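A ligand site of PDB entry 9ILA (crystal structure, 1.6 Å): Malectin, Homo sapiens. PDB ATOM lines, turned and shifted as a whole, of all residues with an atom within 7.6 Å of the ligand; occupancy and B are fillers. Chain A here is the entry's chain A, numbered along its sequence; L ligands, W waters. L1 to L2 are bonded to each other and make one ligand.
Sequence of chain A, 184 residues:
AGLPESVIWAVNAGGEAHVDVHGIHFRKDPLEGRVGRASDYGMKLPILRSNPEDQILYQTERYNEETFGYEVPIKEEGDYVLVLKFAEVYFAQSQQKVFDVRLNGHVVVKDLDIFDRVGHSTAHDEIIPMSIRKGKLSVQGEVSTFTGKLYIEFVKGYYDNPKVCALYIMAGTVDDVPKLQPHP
O3 of LIG L1 is in hydrogen-bond range of OD1 of Asp 160.
An oxygen (O3) of LG2 L2 sits at hydrogen-bond distance from the side-chain carboxylate (OE2) of Glu 61.
NZ of Lys 97 is in hydrogen-bond range of O2 of LG2 L2 (2.9 Å).
The side-chain amide nitrogen of Asn 161 lies within hydrogen-bond range of an oxygen (O1) of LG2 L2 (3.1 Å).
The side-chain hydroxyl of Ser 39 is in hydrogen-bond range of an oxygen (O5) of LG2 L2 (2.7 Å).
O of Glu 61 is in hydrogen-bond range of N of Ser 39.
O of Ala 87 is in hydrogen-bond range of NZ of Lys 163 (2.8 Å).
O of Asn 161 lies within hydrogen-bond range of NZ of Lys 97 (2.9 Å).
The side-chain carboxylate (OD2) of Asp 160 is in salt-bridge range of the side-chain amino group (NZ) of Lys 97, 2.9 Å away.
The side-chain hydroxyl of Ser 39 sits at hydrogen-bond distance from the backbone NH of Tyr 41 (3.1 Å).
The backbone NH (N) of Tyr 90 is in hydrogen-bond range of the side-chain carboxylate (OE2) of Glu 88.
The side-chain carboxylate (OE1) of Glu 61 lies within salt-bridge range of the side-chain amino group (NZ) of Lys 163 (3.1 Å).
O of Tyr 63 sits at hydrogen-bond distance from N of Arg 37 (2.9 Å).
Residues that only touch the ligand: Tyr 41 (3.6 Å), Tyr 63 (3.7 Å), Val 89 (3.6 Å), Tyr 90 (3.6 Å) and Lys 163 (3.9 Å).
Hydrophobic or aromatic side chains within 4 Å of the ligand: Tyr 41, Tyr 63, Val 89 and Tyr 90.
Ten residues have an atom within 4 Å of the ligand: Ser 39, Tyr 41, Glu 61, Tyr 63, Val 89, Tyr 90, Lys 97, Asp 160, Asn 161 and Lys 163.
The nearest printed residue that does not touch the ligand is Phe 91 (4.5 Å).
Water W4 lies within hydrogen-bond range of OE2 of Glu 88, O3 of LG2 L2, NZ of Lys 163 and N of Val 89.
Water W1 lies within hydrogen-bond range of the side-chain amide nitrogen of Asn 161 (3.0 Å) and an oxygen (O3) of LIG L1 (3.1 Å).
Water W6 bridges the side-chain hydroxyl (OH) of Tyr 90 (2.9 Å) and an oxygen (O1) of LIG L1 (3.4 Å).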
ATOM      1  N   ARG A  37      -3.356 -10.061 -13.291  1.00  0.00           N
ATOM      2  CA  ARG A  37      -4.476 -10.341 -12.393  1.00  0.00           C
ATOM      3  C   ARG A  37      -5.759 -10.583 -13.173  1.00  0.00           C
ATOM      4  O   ARG A  37      -6.174  -9.729 -13.959  1.00  0.00           O
ATOM      5  CB  ARG A  37      -4.711  -9.183 -11.436  1.00  0.00           C
ATOM      6  CG  ARG A  37      -3.458  -8.482 -11.029  1.00  0.00           C
ATOM      7  CD  ARG A  37      -3.744  -7.435 -10.001  1.00  0.00           C
ATOM      8  NE  ARG A  37      -2.542  -7.128  -9.253  1.00  0.00           N
ATOM      9  CZ  ARG A  37      -2.184  -7.745  -8.135  1.00  0.00           C
ATOM     10  NH1 ARG A  37      -2.973  -8.644  -7.558  1.00  0.00           N
ATOM     11  NH2 ARG A  37      -1.015  -7.457  -7.575  1.00  0.00           N
ATOM     12  N   ALA A  38      -6.410 -11.724 -12.911  1.00  0.00           N
ATOM     13  CA  ALA A  38      -7.726 -12.001 -13.474  1.00  0.00           C
ATOM     14  C   ALA A  38      -8.827 -11.258 -12.714  1.00  0.00           C
ATOM     15  O   ALA A  38      -8.755 -11.105 -11.489  1.00  0.00           O
ATOM     16  CB  ALA A  38      -8.022 -13.511 -13.422  1.00  0.00           C
ATOM     17  N   SER A  39      -9.843 -10.771 -13.457  1.00  0.00           N
ATOM     18  CA  SER A  39     -11.016 -10.156 -12.829  1.00  0.00           C
ATOM     19  C   SER A  39     -12.297 -10.510 -13.584  1.00  0.00           C
ATOM     20  O   SER A  39     -12.371 -10.337 -14.811  1.00  0.00           O
ATOM     21  CB  SER A  39     -10.894  -8.629 -12.748  1.00  0.00           C
ATOM     22  OG  SER A  39     -12.126  -8.070 -12.270  1.00  0.00           O
ATOM     23  N   ASP A  40     -13.312 -10.974 -12.838  1.00  0.00           N
ATOM     24  CA  ASP A  40     -14.665 -11.197 -13.357  1.00  0.00           C
ATOM     25  C   ASP A  40     -15.639 -10.085 -12.944  1.00  0.00           C
ATOM     26  O   ASP A  40     -16.863 -10.325 -12.926  1.00  0.00           O
ATOM     27  CB  ASP A  40     -15.183 -12.564 -12.930  1.00  0.00           C
ATOM     28  CG  ASP A  40     -15.388 -12.678 -11.427  1.00  0.00           C
ATOM     29  OD1 ASP A  40     -15.061 -11.734 -10.678  1.00  0.00           O
ATOM     30  OD2 ASP A  40     -15.870 -13.752 -10.989  1.00  0.00           O
ATOM     31  N   TYR A  41     -15.128  -8.884 -12.656  1.00  0.00           N
ATOM     32  CA  TYR A  41     -15.989  -7.759 -12.238  1.00  0.00           C
ATOM     33  C   TYR A  41     -17.083  -7.465 -13.261  1.00  0.00           C
ATOM     34  O   TYR A  41     -18.221  -7.132 -12.897  1.00  0.00           O
ATOM     35  CB  TYR A  41     -15.116  -6.505 -11.995  1.00  0.00           C
ATOM     36  CG  TYR A  41     -15.906  -5.283 -11.542  1.00  0.00           C
ATOM     37  CD1 TYR A  41     -16.322  -5.147 -10.215  1.00  0.00           C
ATOM     38  CD2 TYR A  41     -16.266  -4.275 -12.430  1.00  0.00           C
ATOM     39  CE1 TYR A  41     -17.067  -4.049  -9.784  1.00  0.00           C
ATOM     40  CE2 TYR A  41     -17.009  -3.157 -12.007  1.00  0.00           C
ATOM     41  CZ  TYR A  41     -17.403  -3.057 -10.680  1.00  0.00           C
ATOM     42  OH  TYR A  41     -18.147  -1.969 -10.263  1.00  0.00           O
ATOM     43  N   GLY A  42     -16.778  -7.582 -14.558  1.00  0.00           N
ATOM     44  CA  GLY A  42     -17.764  -7.256 -15.590  1.00  0.00           C
ATOM     45  C   GLY A  42     -18.937  -8.233 -15.711  1.00  0.00           C
ATOM     46  O   GLY A  42     -19.855  -7.962 -16.499  1.00  0.00           O
ATOM     47  N   GLU A  61     -11.433 -10.356 -17.821  1.00  0.00           N
ATOM     48  CA  GLU A  61     -10.221  -9.664 -18.263  1.00  0.00           C
ATOM     49  C   GLU A  61      -8.978 -10.155 -17.502  1.00  0.00           C
ATOM     50  O   GLU A  61      -9.074 -10.722 -16.414  1.00  0.00           O
ATOM     51  CB  GLU A  61     -10.329  -8.132 -18.071  1.00  0.00           C
ATOM     52  CG  GLU A  61     -10.271  -7.693 -16.577  1.00  0.00           C
ATOM     53  CD  GLU A  61     -10.605  -6.207 -16.345  1.00  0.00           C
ATOM     54  OE1 GLU A  61      -9.740  -5.359 -16.658  1.00  0.00           O
ATOM     55  OE2 GLU A  61     -11.717  -5.907 -15.834  1.00  0.00           O
ATOM     56  N   ARG A  62      -7.796  -9.869 -18.085  1.00  0.00           N
ATOM     57  CA  ARG A  62      -6.521  -9.823 -17.357  1.00  0.00           C
ATOM     58  C   ARG A  62      -5.950  -8.400 -17.457  1.00  0.00           C
ATOM     59  O   ARG A  62      -5.882  -7.839 -18.557  1.00  0.00           O
ATOM     60  CB  ARG A  62      -5.512 -10.848 -17.924  1.00  0.00           C
ATOM     61  CG  ARG A  62      -4.160 -10.908 -17.149  1.00  0.00           C
ATOM     62  CD  ARG A  62      -3.337 -12.213 -17.417  1.00  0.00           C
ATOM     63  NE  ARG A  62      -4.081 -13.380 -16.949  1.00  0.00           N
ATOM     64  CZ  ARG A  62      -4.114 -13.800 -15.693  1.00  0.00           C
ATOM     65  NH1 ARG A  62      -3.306 -13.296 -14.770  1.00  0.00           N
ATOM     66  NH2 ARG A  62      -4.995 -14.732 -15.341  1.00  0.00           N
ATOM     67  N   TYR A  63      -5.544  -7.822 -16.306  1.00  0.00           N
ATOM     68  CA  TYR A  63      -4.936  -6.482 -16.243  1.00  0.00           C
ATOM     69  C   TYR A  63      -3.695  -6.512 -15.346  1.00  0.00           C
ATOM     70  O   TYR A  63      -3.450  -7.495 -14.642  1.00  0.00           O
ATOM     71  CB  TYR A  63      -5.951  -5.418 -15.754  1.00  0.00           C
ATOM     72  CG  TYR A  63      -6.235  -5.396 -14.256  1.00  0.00           C
ATOM     73  CD1 TYR A  63      -7.263  -6.161 -13.700  1.00  0.00           C
ATOM     74  CD2 TYR A  63      -5.496  -4.580 -13.394  1.00  0.00           C
ATOM     75  CE1 TYR A  63      -7.529  -6.137 -12.331  1.00  0.00           C
ATOM     76  CE2 TYR A  63      -5.748  -4.554 -12.027  1.00  0.00           C
ATOM     77  CZ  TYR A  63      -6.770  -5.328 -11.506  1.00  0.00           C
ATOM     78  OH  TYR A  63      -7.030  -5.303 -10.145  1.00  0.00           O
ATOM     79  N   ASN A  64      -2.903  -5.431 -15.354  1.00  0.00           N
ATOM     80  CA  ASN A  64      -1.707  -5.369 -14.506  1.00  0.00           C
ATOM     81  C   ASN A  64      -1.252  -3.926 -14.292  1.00  0.00           C
ATOM     82  O   ASN A  64      -1.494  -3.057 -15.143  1.00  0.00           O
ATOM     83  CB  ASN A  64      -0.552  -6.202 -15.105  1.00  0.00           C
ATOM     84  CG  ASN A  64       0.479  -6.671 -14.058  1.00  0.00           C
ATOM     85  OD1 ASN A  64       0.126  -7.036 -12.942  1.00  0.00           O
ATOM     86  ND2 ASN A  64       1.748  -6.702 -14.462  1.00  0.00           N
ATOM     87  N   GLU A  65      -0.563  -3.678 -13.169  1.00  0.00           N
ATOM     88  CA  GLU A  65       0.019  -2.361 -12.869  1.00  0.00           C
ATOM     89  C   GLU A  65       1.387  -2.160 -13.507  1.00  0.00           C
ATOM     90  O   GLU A  65       1.952  -1.052 -13.399  1.00  0.00           O
ATOM     91  CB  GLU A  65       0.129  -2.166 -11.344  1.00  0.00           C
ATOM     92  CG  GLU A  65      -1.218  -1.974 -10.626  1.00  0.00           C
ATOM     93  CD  GLU A  65      -1.060  -1.739  -9.134  1.00  0.00           C
ATOM     94  OE1 GLU A  65      -1.706  -2.463  -8.331  1.00  0.00           O
ATOM     95  OE2 GLU A  65      -0.309  -0.824  -8.744  1.00  0.00           O
ATOM     96  N   ALA A  87     -13.180  -4.253 -23.515  1.00  0.00           N
ATOM     97  CA  ALA A  87     -14.297  -3.454 -22.982  1.00  0.00           C
ATOM     98  C   ALA A  87     -13.834  -2.690 -21.742  1.00  0.00           C
ATOM     99  O   ALA A  87     -13.041  -3.201 -20.952  1.00  0.00           O
ATOM    100  CB  ALA A  87     -15.523  -4.324 -22.620  1.00  0.00           C
ATOM    101  N   GLU A  88     -14.374  -1.461 -21.565  1.00  0.00           N
ATOM    102  CA  GLU A  88     -14.118  -0.648 -20.345  1.00  0.00           C
ATOM    103  C   GLU A  88     -15.281  -0.833 -19.376  1.00  0.00           C
ATOM    104  O   GLU A  88     -16.373  -0.284 -19.582  1.00  0.00           O
ATOM    105  CB  GLU A  88     -13.906   0.820 -20.709  1.00  0.00           C
ATOM    106  CG  GLU A  88     -13.701   1.776 -19.497  1.00  0.00           C
ATOM    107  CD  GLU A  88     -12.478   1.415 -18.653  1.00  0.00           C
ATOM    108  OE1 GLU A  88     -11.315   1.627 -19.119  1.00  0.00           O
ATOM    109  OE2 GLU A  88     -12.687   0.886 -17.521  1.00  0.00           O
ATOM    110  N   VAL A  89     -15.053  -1.610 -18.300  1.00  0.00           N
ATOM    111  CA  VAL A  89     -16.123  -1.940 -17.355  1.00  0.00           C
ATOM    112  C   VAL A  89     -16.010  -1.135 -16.046  1.00  0.00           C
ATOM    113  O   VAL A  89     -16.746  -1.427 -15.093  1.00  0.00           O
ATOM    114  CB  VAL A  89     -16.178  -3.469 -17.065  1.00  0.00           C
ATOM    115  CG1 VAL A  89     -16.532  -4.252 -18.349  1.00  0.00           C
ATOM    116  CG2 VAL A  89     -14.891  -4.003 -16.406  1.00  0.00           C
ATOM    117  N   TYR A  90     -15.134  -0.117 -15.995  1.00  0.00           N
ATOM    118  CA  TYR A  90     -14.995   0.703 -14.766  1.00  0.00           C
ATOM    119  C   TYR A  90     -15.152   2.219 -15.025  1.00  0.00           C
ATOM    120  O   TYR A  90     -16.027   2.843 -14.435  1.00  0.00           O
ATOM    121  CB  TYR A  90     -13.650   0.436 -14.055  1.00  0.00           C
ATOM    122  CG  TYR A  90     -13.562   1.013 -12.645  1.00  0.00           C
ATOM    123  CD1 TYR A  90     -14.239   0.408 -11.574  1.00  0.00           C
ATOM    124  CD2 TYR A  90     -12.836   2.186 -12.367  1.00  0.00           C
ATOM    125  CE1 TYR A  90     -14.144   0.944 -10.270  1.00  0.00           C
ATOM    126  CE2 TYR A  90     -12.764   2.718 -11.082  1.00  0.00           C
ATOM    127  CZ  TYR A  90     -13.411   2.098 -10.042  1.00  0.00           C
ATOM    128  OH  TYR A  90     -13.337   2.650  -8.765  1.00  0.00           O
ATOM    129  N   PHE A  91     -14.347   2.802 -15.913  1.00  0.00           N
ATOM    130  CA  PHE A  91     -14.365   4.244 -16.159  1.00  0.00           C
ATOM    131  C   PHE A  91     -15.433   4.645 -17.208  1.00  0.00           C
ATOM    132  O   PHE A  91     -15.901   3.835 -18.014  1.00  0.00           O
ATOM    133  CB  PHE A  91     -12.984   4.736 -16.622  1.00  0.00           C
ATOM    134  CG  PHE A  91     -11.901   4.583 -15.575  1.00  0.00           C
ATOM    135  CD1 PHE A  91     -11.819   5.451 -14.478  1.00  0.00           C
ATOM    136  CD2 PHE A  91     -10.946   3.583 -15.685  1.00  0.00           C
ATOM    137  CE1 PHE A  91     -10.818   5.312 -13.509  1.00  0.00           C
ATOM    138  CE2 PHE A  91      -9.941   3.424 -14.716  1.00  0.00           C
ATOM    139  CZ  PHE A  91      -9.885   4.307 -13.625  1.00  0.00           C
ATOM    140  N   LYS A  97      -8.011   5.639 -18.578  1.00  0.00           N
ATOM    141  CA  LYS A  97      -7.175   4.469 -18.880  1.00  0.00           C
ATOM    142  C   LYS A  97      -6.721   4.554 -20.337  1.00  0.00           C
ATOM    143  O   LYS A  97      -7.556   4.576 -21.251  1.00  0.00           O
ATOM    144  CB  LYS A  97      -7.944   3.161 -18.626  1.00  0.00           C
ATOM    145  CG  LYS A  97      -7.178   1.854 -18.982  1.00  0.00           C
ATOM    146  CD  LYS A  97      -8.106   0.611 -19.072  1.00  0.00           C
ATOM    147  CE  LYS A  97      -8.714   0.177 -17.720  1.00  0.00           C
ATOM    148  NZ  LYS A  97      -7.710  -0.360 -16.734  1.00  0.00           N
ATOM    149  N   ASP A 160      -3.724   4.851 -15.593  1.00  0.00           N
ATOM    150  CA  ASP A 160      -4.267   3.572 -15.080  1.00  0.00           C
ATOM    151  C   ASP A 160      -3.550   2.373 -15.748  1.00  0.00           C
ATOM    152  O   ASP A 160      -2.377   2.466 -16.119  1.00  0.00           O
ATOM    153  CB  ASP A 160      -5.788   3.555 -15.209  1.00  0.00           C
ATOM    154  CG  ASP A 160      -6.438   2.566 -14.228  1.00  0.00           C
ATOM    155  OD1 ASP A 160      -6.491   2.897 -13.027  1.00  0.00           O
ATOM    156  OD2 ASP A 160      -6.877   1.460 -14.637  1.00  0.00           O
ATOM    157  N   ASN A 161      -4.252   1.237 -15.908  1.00  0.00           N
ATOM    158  CA  ASN A 161      -3.611  -0.073 -16.120  1.00  0.00           C
ATOM    159  C   ASN A 161      -3.950  -0.681 -17.481  1.00  0.00           C
ATOM    160  O   ASN A 161      -5.124  -0.702 -17.885  1.00  0.00           O
ATOM    161  CB  ASN A 161      -4.036  -1.086 -15.021  1.00  0.00           C
ATOM    162  CG  ASN A 161      -3.687  -0.608 -13.594  1.00  0.00           C
ATOM    163  OD1 ASN A 161      -2.626  -0.030 -13.353  1.00  0.00           O
ATOM    164  ND2 ASN A 161      -4.582  -0.913 -12.656  1.00  0.00           N
ATOM    165  N   PRO A 162      -2.953  -1.241 -18.181  1.00  0.00           N
ATOM    166  CA  PRO A 162      -3.246  -2.021 -19.413  1.00  0.00           C
ATOM    167  C   PRO A 162      -4.066  -3.278 -19.128  1.00  0.00           C
ATOM    168  O   PRO A 162      -3.955  -3.874 -18.055  1.00  0.00           O
ATOM    169  CB  PRO A 162      -1.843  -2.373 -19.953  1.00  0.00           C
ATOM    170  CG  PRO A 162      -0.957  -2.369 -18.703  1.00  0.00           C
ATOM    171  CD  PRO A 162      -1.512  -1.217 -17.869  1.00  0.00           C
ATOM    172  N   LYS A 163      -4.898  -3.685 -20.108  1.00  0.00           N
ATOM    173  CA  LYS A 163      -5.805  -4.829 -19.983  1.00  0.00           C
ATOM    174  C   LYS A 163      -6.122  -5.442 -21.353  1.00  0.00           C
ATOM    175  O   LYS A 163      -5.926  -4.813 -22.401  1.00  0.00           O
ATOM    176  CB  LYS A 163      -7.118  -4.426 -19.281  1.00  0.00           C
ATOM    177  CG  LYS A 163      -8.059  -3.537 -20.134  1.00  0.00           C
ATOM    178  CD  LYS A 163      -9.441  -3.343 -19.485  1.00  0.00           C
ATOM    179  CE  LYS A 163     -10.350  -4.573 -19.676  1.00  0.00           C
ATOM    180  NZ  LYS A 163     -11.642  -4.450 -18.897  1.00  0.00           N
ATOM    181  N   VAL A 164      -6.627  -6.689 -21.341  1.00  0.00           N
ATOM    182  CA  VAL A 164      -7.186  -7.350 -22.527  1.00  0.00           C
ATOM    183  C   VAL A 164      -8.290  -8.326 -22.093  1.00  0.00           C
ATOM    184  O   VAL A 164      -8.225  -8.901 -21.003  1.00  0.00           O
ATOM    185  CB  VAL A 164      -6.073  -8.041 -23.361  1.00  0.00           C
ATOM    186  CG1 VAL A 164      -5.517  -9.255 -22.632  1.00  0.00           C
ATOM    187  CG2 VAL A 164      -6.589  -8.460 -24.749  1.00  0.00           C
HETATM  188  C1  LIG L   1      -8.316   1.925  -9.457  1.00  0.00           C
HETATM  189  C2  LIG L   1      -8.475   1.111 -10.741  1.00  0.00           C
HETATM  190  C3  LIG L   1      -9.204  -0.209 -10.469  1.00  0.00           C
HETATM  191  C4  LIG L   1     -10.499   0.065  -9.708  1.00  0.00           C
HETATM  192  C5  LIG L   1     -11.260  -1.177  -9.279  1.00  0.00           C
HETATM  193  C6  LIG L   1      -9.661   2.097  -8.768  1.00  0.00           C
HETATM  194  O1  LIG L   1      -9.508   2.797  -7.572  1.00  0.00           O
HETATM  195  O2  LIG L   1      -7.762   3.209  -9.751  1.00  0.00           O
HETATM  196  O3  LIG L   1      -7.198   0.854 -11.331  1.00  0.00           O
HETATM  197  O4  LIG L   1      -9.470  -0.841 -11.721  1.00  0.00           O
HETATM  198  O5  LIG L   1     -10.224   0.811  -8.509  1.00  0.00           O
HETATM  199  O6  LIG L   1     -10.471  -1.985  -8.409  1.00  0.00           O
HETATM  200  C1  LG2 L   2      -8.973  -2.201 -11.863  1.00  0.00           C
HETATM  201  C2  LG2 L   2      -8.482  -2.405 -13.308  1.00  0.00           C
HETATM  202  C3  LG2 L   2      -9.627  -2.397 -14.339  1.00  0.00           C
HETATM  203  C4  LG2 L   2     -10.679  -3.403 -13.880  1.00  0.00           C
HETATM  204  C5  LG2 L   2     -11.111  -3.137 -12.427  1.00  0.00           C
HETATM  205  C6  LG2 L   2     -12.177  -4.135 -11.939  1.00  0.00           C
HETATM  206  O1  LG2 L   2      -7.501  -1.411 -13.619  1.00  0.00           O
HETATM  207  O2  LG2 L   2      -9.141  -2.702 -15.660  1.00  0.00           O
HETATM  208  O3  LG2 L   2     -11.804  -3.400 -14.750  1.00  0.00           O
HETATM  209  O4  LG2 L   2      -9.983  -3.160 -11.557  1.00  0.00           O
HETATM  210  O5  LG2 L   2     -11.638  -5.431 -11.774  1.00  0.00           O
HETATM  211  O   HOH W   1      -4.971  -0.557  -9.712  1.00  0.00           O
HETATM  212  O   HOH W   2      -4.644   3.185  -9.753  1.00  0.00           O
HETATM  213  O   HOH W   3      -9.595   5.555 -10.093  1.00  0.00           O
HETATM  214  O   HOH W   4     -12.137  -1.909 -17.335  1.00  0.00           O
HETATM  215  O   HOH W   5      -8.071  -1.573  -6.687  1.00  0.00           O
HETATM  216  O   HOH W   6     -11.922   5.113  -8.102  1.00  0.00           O
